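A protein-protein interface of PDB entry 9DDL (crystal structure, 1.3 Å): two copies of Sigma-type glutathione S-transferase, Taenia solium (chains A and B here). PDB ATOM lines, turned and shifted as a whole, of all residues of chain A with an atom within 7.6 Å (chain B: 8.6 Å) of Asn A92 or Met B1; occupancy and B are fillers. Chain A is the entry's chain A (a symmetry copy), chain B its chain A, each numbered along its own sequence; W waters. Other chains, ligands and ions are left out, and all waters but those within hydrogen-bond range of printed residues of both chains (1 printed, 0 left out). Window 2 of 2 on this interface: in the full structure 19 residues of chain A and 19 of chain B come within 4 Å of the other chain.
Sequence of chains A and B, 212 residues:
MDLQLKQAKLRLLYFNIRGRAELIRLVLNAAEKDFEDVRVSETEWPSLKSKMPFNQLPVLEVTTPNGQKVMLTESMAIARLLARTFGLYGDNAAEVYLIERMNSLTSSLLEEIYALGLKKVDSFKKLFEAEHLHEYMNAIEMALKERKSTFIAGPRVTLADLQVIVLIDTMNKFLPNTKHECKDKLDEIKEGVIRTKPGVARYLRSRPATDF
CE of Met B1 touches ND2 of Asn A92, at 3.7 Å. Ala A93 touches Leu B81 (O to CD1, 3.8 Å). CB of Ala A94 touches O of Met B1, at 3.1 Å. Val A96 touches Arg B84. OH of Tyr A97 touches CA of Leu B72, at 3.6 Å. Leu B81 touches Tyr A97 (CD2 to CD1, 3.9 Å).
Printed residues of chain B that touch a printed residue of chain A: Met B1, Leu B72, Leu B81 and Arg B84. Hydrophobic or aromatic side chains of chain B within 4 Å of the printed part of chain A: Met B1, Leu B72 and Leu B81. Among the printed residues, 6 pairs touch across the chains. Among the printed residues, no Asp or Glu carboxylate lies within 4 Å of a Lys or Arg side-chain nitrogen of the other chain.
Of the printed residues of chain B, Asn A92 touches Met B1 (3.7 Å). Of the printed residues of chain A, Met B1 touches Asn A92 (3.7 Å) and Ala A94 (3.1 Å). Ala A93 touches just one residue of chain B: Leu B81 (3.8 Å). Printed residues of chain A within 4 Å of Arg B84: Val A96 (3.4 Å). Of the printed residues of chain A, Leu B81 touches Ala A93 and Tyr A97. Of the printed residues of chain B, Val A96 touches Arg B84 (3.4 Å). Of the printed residues of chain A, Leu B72 touches Tyr A97. Of the printed residues of chain B, Ala A94 touches Met B1 (3.1 Å). Asp B2 touches none of the printed residues of chain A.
The side-chain amide oxygen (OD1) of Asn A92 lies close to the backbone NH (N) of Ala A94 (3.2 Å). N of Glu A95 sits at hydrogen-bond distance from OD1 of Asn A92 (2.9 Å).
No position is printed for both chains. Of the 6 pairs that touch across the chains among the printed residues, none has its exchanged pair printed and touching as well.
Water W1 bridges NH1 of Arg B84 (2.8 Å) and O of Ala A93 (2.9 Å).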
ATOM      1  N   TYR A  89       0.326  -5.509 -25.032  1.00  0.00           N
ATOM      2  CA  TYR A  89       1.753  -5.541 -25.332  1.00  0.00           C
ATOM      3  C   TYR A  89       2.189  -4.388 -26.226  1.00  0.00           C
ATOM      4  O   TYR A  89       3.140  -4.529 -27.005  1.00  0.00           O
ATOM      5  CB  TYR A  89       2.183  -6.895 -25.905  1.00  0.00           C
ATOM      6  CG  TYR A  89       3.594  -7.257 -25.493  1.00  0.00           C
ATOM      7  CD1 TYR A  89       3.894  -7.615 -24.171  1.00  0.00           C
ATOM      8  CD2 TYR A  89       4.632  -7.244 -26.415  1.00  0.00           C
ATOM      9  CE1 TYR A  89       5.188  -7.920 -23.763  1.00  0.00           C
ATOM     10  CE2 TYR A  89       5.945  -7.565 -26.003  1.00  0.00           C
ATOM     11  CZ  TYR A  89       6.206  -7.896 -24.676  1.00  0.00           C
ATOM     12  OH  TYR A  89       7.485  -8.195 -24.273  1.00  0.00           O
ATOM     13  N   GLY A  90       1.518  -3.246 -26.116  1.00  0.00           N
ATOM     14  CA  GLY A  90       1.905  -2.061 -26.873  1.00  0.00           C
ATOM     15  C   GLY A  90       1.597  -2.160 -28.353  1.00  0.00           C
ATOM     16  O   GLY A  90       1.056  -3.141 -28.851  1.00  0.00           O
ATOM     17  N   ASP A  91       1.988  -1.095 -29.070  1.00  0.00           N
ATOM     18  CA  ASP A  91       1.611  -0.901 -30.464  1.00  0.00           C
ATOM     19  C   ASP A  91       2.792  -0.802 -31.414  1.00  0.00           C
ATOM     20  O   ASP A  91       2.585  -0.869 -32.631  1.00  0.00           O
ATOM     21  CB  ASP A  91       0.784   0.384 -30.626  1.00  0.00           C
ATOM     22  CG  ASP A  91      -0.471   0.368 -29.798  1.00  0.00           C
ATOM     23  OD1 ASP A  91      -1.145  -0.684 -29.783  1.00  0.00           O
ATOM     24  OD2 ASP A  91      -0.777   1.401 -29.163  1.00  0.00           O
ATOM     25  N   ASN A  92       4.010  -0.644 -30.907  1.00  0.00           N
ATOM     26  CA  ASN A  92       5.179  -0.528 -31.764  1.00  0.00           C
ATOM     27  C   ASN A  92       6.402  -0.947 -30.971  1.00  0.00           C
ATOM     28  O   ASN A  92       6.341  -1.155 -29.755  1.00  0.00           O
ATOM     29  CB  ASN A  92       5.318   0.890 -32.322  1.00  0.00           C
ATOM     30  CG  ASN A  92       5.329   1.932 -31.247  1.00  0.00           C
ATOM     31  OD1 ASN A  92       6.158   1.906 -30.349  1.00  0.00           O
ATOM     32  ND2 ASN A  92       4.417   2.895 -31.347  1.00  0.00           N
ATOM     33  N   ALA A  93       7.522  -1.080 -31.686  1.00  0.00           N
ATOM     34  CA  ALA A  93       8.724  -1.639 -31.068  1.00  0.00           C
ATOM     35  C   ALA A  93       9.289  -0.722 -29.995  1.00  0.00           C
ATOM     36  O   ALA A  93       9.920  -1.198 -29.044  1.00  0.00           O
ATOM     37  CB  ALA A  93       9.787  -1.929 -32.131  1.00  0.00           C
ATOM     38  N   ALA A  94       9.088   0.590 -30.131  1.00  0.00           N
ATOM     39  CA  ALA A  94       9.587   1.514 -29.117  1.00  0.00           C
ATOM     40  C   ALA A  94       8.840   1.341 -27.806  1.00  0.00           C
ATOM     41  O   ALA A  94       9.452   1.297 -26.726  1.00  0.00           O
ATOM     42  CB  ALA A  94       9.459   2.951 -29.614  1.00  0.00           C
ATOM     43  N   GLU A  95       7.506   1.231 -27.870  1.00  0.00           N
ATOM     44  CA  GLU A  95       6.736   0.925 -26.664  1.00  0.00           C
ATOM     45  C   GLU A  95       7.136  -0.420 -26.084  1.00  0.00           C
ATOM     46  O   GLU A  95       7.243  -0.573 -24.858  1.00  0.00           O
ATOM     47  CB  GLU A  95       5.241   0.926 -26.978  1.00  0.00           C
ATOM     48  CG  GLU A  95       4.744   2.292 -27.380  1.00  0.00           C
ATOM     49  CD  GLU A  95       3.255   2.328 -27.638  1.00  0.00           C
ATOM     50  OE1 GLU A  95       2.582   1.283 -27.500  1.00  0.00           O
ATOM     51  OE2 GLU A  95       2.763   3.418 -27.992  1.00  0.00           O
ATOM     52  N   VAL A  96       7.378  -1.405 -26.947  1.00  0.00           N
ATOM     53  CA  VAL A  96       7.748  -2.729 -26.467  1.00  0.00           C
ATOM     54  C   VAL A  96       9.101  -2.680 -25.778  1.00  0.00           C
ATOM     55  O   VAL A  96       9.325  -3.394 -24.799  1.00  0.00           O
ATOM     56  CB  VAL A  96       7.702  -3.768 -27.602  1.00  0.00           C
ATOM     57  CG1 VAL A  96       8.253  -5.099 -27.128  1.00  0.00           C
ATOM     58  CG2 VAL A  96       6.268  -3.940 -28.065  1.00  0.00           C
ATOM     59  N   TYR A  97      10.027  -1.843 -26.261  1.00  0.00           N
ATOM     60  CA  TYR A  97      11.287  -1.698 -25.534  1.00  0.00           C
ATOM     61  C   TYR A  97      11.039  -1.240 -24.096  1.00  0.00           C
ATOM     62  O   TYR A  97      11.667  -1.748 -23.145  1.00  0.00           O
ATOM     63  CB  TYR A  97      12.253  -0.740 -26.267  1.00  0.00           C
ATOM     64  CG  TYR A  97      13.465  -0.514 -25.408  1.00  0.00           C
ATOM     65  CD1 TYR A  97      14.465  -1.493 -25.286  1.00  0.00           C
ATOM     66  CD2 TYR A  97      13.559   0.619 -24.617  1.00  0.00           C
ATOM     67  CE1 TYR A  97      15.545  -1.324 -24.412  1.00  0.00           C
ATOM     68  CE2 TYR A  97      14.626   0.802 -23.750  1.00  0.00           C
ATOM     69  CZ  TYR A  97      15.603  -0.160 -23.644  1.00  0.00           C
ATOM     70  OH  TYR A  97      16.643   0.075 -22.747  1.00  0.00           O
ATOM     71  N   LEU A  98      10.140  -0.270 -23.902  1.00  0.00           N
ATOM     72  CA  LEU A  98       9.824   0.163 -22.546  1.00  0.00           C
ATOM     73  C   LEU A  98       9.255  -0.984 -21.721  1.00  0.00           C
ATOM     74  O   LEU A  98       9.615  -1.145 -20.540  1.00  0.00           O
ATOM     75  CB  LEU A  98       8.849   1.346 -22.572  1.00  0.00           C
ATOM     76  CG  LEU A  98       9.450   2.597 -23.200  1.00  0.00           C
ATOM     77  CD1 LEU A  98       8.413   3.733 -23.210  1.00  0.00           C
ATOM     78  CD2 LEU A  98      10.718   3.035 -22.467  1.00  0.00           C
ATOM     79  N   ILE A  99       8.353  -1.783 -22.306  1.00  0.00           N
ATOM     80  CA  ILE A  99       7.814  -2.942 -21.588  1.00  0.00           C
ATOM     81  C   ILE A  99       8.937  -3.873 -21.175  1.00  0.00           C
ATOM     82  O   ILE A  99       8.997  -4.340 -20.029  1.00  0.00           O
ATOM     83  CB  ILE A  99       6.801  -3.696 -22.469  1.00  0.00           C
ATOM     84  CG1 ILE A  99       5.589  -2.837 -22.810  1.00  0.00           C
ATOM     85  CG2 ILE A  99       6.398  -5.009 -21.826  1.00  0.00           C
ATOM     86  CD1 ILE A  99       4.621  -3.523 -23.817  1.00  0.00           C
ATOM     87  N   ALA A 153       4.662   1.958 -20.249  1.00  0.00           N
ATOM     88  CA  ALA A 153       5.023   2.017 -21.658  1.00  0.00           C
ATOM     89  C   ALA A 153       4.138   2.958 -22.446  1.00  0.00           C
ATOM     90  O   ALA A 153       4.256   3.036 -23.676  1.00  0.00           O
ATOM     91  CB  ALA A 153       5.079   0.621 -22.277  1.00  0.00           C
ATOM     92  N   MET B   1      10.383   9.109 -29.569  1.00  0.00           N
ATOM     93  CA  MET B   1      10.018   7.763 -29.144  1.00  0.00           C
ATOM     94  C   MET B   1      10.579   6.707 -30.102  1.00  0.00           C
ATOM     95  O   MET B   1      11.032   5.655 -29.665  1.00  0.00           O
ATOM     96  CB  MET B   1       8.498   7.638 -28.971  1.00  0.00           C
ATOM     97  CG  MET B   1       8.012   6.265 -28.519  1.00  0.00           C
ATOM     98  SD  MET B   1       6.295   5.919 -28.974  1.00  0.00           S
ATOM     99  CE  MET B   1       6.374   6.012 -30.757  1.00  0.00           C
ATOM    100  N   ASP B   2      10.573   6.999 -31.401  1.00  0.00           N
ATOM    101  CA  ASP B   2      11.228   6.148 -32.396  1.00  0.00           C
ATOM    102  C   ASP B   2      12.667   6.621 -32.571  1.00  0.00           C
ATOM    103  O   ASP B   2      12.908   7.755 -32.984  1.00  0.00           O
ATOM    104  CB  ASP B   2      10.479   6.201 -33.730  1.00  0.00           C
ATOM    105  CG  ASP B   2      11.255   5.555 -34.883  1.00  0.00           C
ATOM    106  OD1 ASP B   2      11.966   4.540 -34.690  1.00  0.00           O
ATOM    107  OD2 ASP B   2      11.150   6.090 -36.007  1.00  0.00           O
ATOM    108  N   LEU B   3      13.623   5.748 -32.266  1.00  0.00           N
ATOM    109  CA  LEU B   3      15.041   6.096 -32.347  1.00  0.00           C
ATOM    110  C   LEU B   3      15.619   6.038 -33.756  1.00  0.00           C
ATOM    111  O   LEU B   3      16.792   6.405 -33.937  1.00  0.00           O
ATOM    112  CB  LEU B   3      15.834   5.169 -31.421  1.00  0.00           C
ATOM    113  CG  LEU B   3      15.491   5.374 -29.930  1.00  0.00           C
ATOM    114  CD1 LEU B   3      16.394   4.570 -29.035  1.00  0.00           C
ATOM    115  CD2 LEU B   3      15.540   6.857 -29.558  1.00  0.00           C
ATOM    116  N   GLN B   4      14.853   5.587 -34.748  1.00  0.00           N
ATOM    117  CA  GLN B   4      15.324   5.515 -36.129  1.00  0.00           C
ATOM    118  C   GLN B   4      16.610   4.701 -36.217  1.00  0.00           C
ATOM    119  O   GLN B   4      17.620   5.145 -36.771  1.00  0.00           O
ATOM    120  CB  GLN B   4      15.513   6.898 -36.752  1.00  0.00           C
ATOM    121  CG  GLN B   4      14.290   7.792 -36.712  1.00  0.00           C
ATOM    122  CD  GLN B   4      14.659   9.227 -37.028  1.00  0.00           C
ATOM    123  OE1 GLN B   4      14.943   9.558 -38.171  1.00  0.00           O
ATOM    124  NE2 GLN B   4      14.694  10.078 -36.000  1.00  0.00           N
ATOM    125  N   LEU B   5      16.550   3.490 -35.665  1.00  0.00           N
ATOM    126  CA  LEU B   5      17.749   2.683 -35.448  1.00  0.00           C
ATOM    127  C   LEU B   5      18.425   2.245 -36.739  1.00  0.00           C
ATOM    128  O   LEU B   5      19.639   2.022 -36.734  1.00  0.00           O
ATOM    129  CB  LEU B   5      17.419   1.472 -34.569  1.00  0.00           C
ATOM    130  CG  LEU B   5      17.012   1.799 -33.123  1.00  0.00           C
ATOM    131  CD1 LEU B   5      16.408   0.586 -32.431  1.00  0.00           C
ATOM    132  CD2 LEU B   5      18.185   2.366 -32.327  1.00  0.00           C
ATOM    133  N   THR B  64      20.450   9.379 -32.503  1.00  0.00           N
ATOM    134  CA  THR B  64      19.462   9.340 -33.571  1.00  0.00           C
ATOM    135  C   THR B  64      19.928  10.208 -34.740  1.00  0.00           C
ATOM    136  O   THR B  64      20.840  11.027 -34.576  1.00  0.00           O
ATOM    137  CB  THR B  64      18.092   9.854 -33.106  1.00  0.00           C
ATOM    138  OG1 THR B  64      18.168  11.271 -32.920  1.00  0.00           O
ATOM    139  CG2 THR B  64      17.623   9.188 -31.826  1.00  0.00           C
ATOM    140  N   GLN B  68      20.028  13.127 -31.201  1.00  0.00           N
ATOM    141  CA  GLN B  68      19.687  12.879 -29.808  1.00  0.00           C
ATOM    142  C   GLN B  68      20.403  11.633 -29.297  1.00  0.00           C
ATOM    143  O   GLN B  68      20.328  10.569 -29.920  1.00  0.00           O
ATOM    144  CB  GLN B  68      18.180  12.704 -29.662  1.00  0.00           C
ATOM    145  CG  GLN B  68      17.772  12.616 -28.188  1.00  0.00           C
ATOM    146  CD  GLN B  68      16.283  12.659 -28.014  1.00  0.00           C
ATOM    147  OE1 GLN B  68      15.560  12.917 -28.972  1.00  0.00           O
ATOM    148  NE2 GLN B  68      15.804  12.395 -26.809  1.00  0.00           N
ATOM    149  N   VAL B  70      20.696   8.677 -26.677  1.00  0.00           N
ATOM    150  CA  VAL B  70      19.878   7.880 -25.767  1.00  0.00           C
ATOM    151  C   VAL B  70      20.686   6.644 -25.389  1.00  0.00           C
ATOM    152  O   VAL B  70      21.238   5.975 -26.266  1.00  0.00           O
ATOM    153  CB  VAL B  70      18.567   7.445 -26.452  1.00  0.00           C
ATOM    154  CG1 VAL B  70      17.729   6.582 -25.508  1.00  0.00           C
ATOM    155  CG2 VAL B  70      17.759   8.659 -26.967  1.00  0.00           C
ATOM    156  N   LEU B  72      20.503   2.956 -24.060  1.00  0.00           N
ATOM    157  CA  LEU B  72      19.607   1.830 -23.833  1.00  0.00           C
ATOM    158  C   LEU B  72      20.280   0.781 -22.964  1.00  0.00           C
ATOM    159  O   LEU B  72      21.469   0.473 -23.140  1.00  0.00           O
ATOM    160  CB  LEU B  72      19.179   1.192 -25.153  1.00  0.00           C
ATOM    161  CG  LEU B  72      18.563   2.124 -26.196  1.00  0.00           C
ATOM    162  CD1 LEU B  72      18.222   1.308 -27.425  1.00  0.00           C
ATOM    163  CD2 LEU B  72      17.318   2.846 -25.648  1.00  0.00           C
ATOM    164  N   LEU B  81      14.727  -5.449 -29.489  1.00  0.00           N
ATOM    165  CA  LEU B  81      14.444  -4.212 -30.210  1.00  0.00           C
ATOM    166  C   LEU B  81      15.197  -4.174 -31.533  1.00  0.00           C
ATOM    167  O   LEU B  81      14.637  -3.808 -32.576  1.00  0.00           O
ATOM    168  CB  LEU B  81      14.853  -3.042 -29.319  1.00  0.00           C
ATOM    169  CG  LEU B  81      14.841  -1.681 -29.997  1.00  0.00           C
ATOM    170  CD1 LEU B  81      13.446  -1.294 -30.521  1.00  0.00           C
ATOM    171  CD2 LEU B  81      15.354  -0.629 -29.019  1.00  0.00           C
ATOM    172  N   ARG B  84      13.688  -6.739 -33.972  1.00  0.00           N
ATOM    173  CA  ARG B  84      12.458  -6.254 -34.584  1.00  0.00           C
ATOM    174  C   ARG B  84      12.758  -5.228 -35.663  1.00  0.00           C
ATOM    175  O   ARG B  84      12.130  -5.235 -36.729  1.00  0.00           O
ATOM    176  CB  ARG B  84      11.565  -5.615 -33.529  1.00  0.00           C
ATOM    177  CG  ARG B  84      10.970  -6.617 -32.561  1.00  0.00           C
ATOM    178  CD  ARG B  84      10.142  -5.915 -31.482  1.00  0.00           C
ATOM    179  NE  ARG B  84       9.563  -6.913 -30.585  1.00  0.00           N
ATOM    180  CZ  ARG B  84      10.001  -7.185 -29.356  1.00  0.00           C
ATOM    181  NH1 ARG B  84      10.940  -6.440 -28.768  1.00  0.00           N
ATOM    182  NH2 ARG B  84       9.469  -8.217 -28.685  1.00  0.00           N
HETATM  183  O   HOH W   1      11.365  -3.666 -28.983  1.00  0.00           O
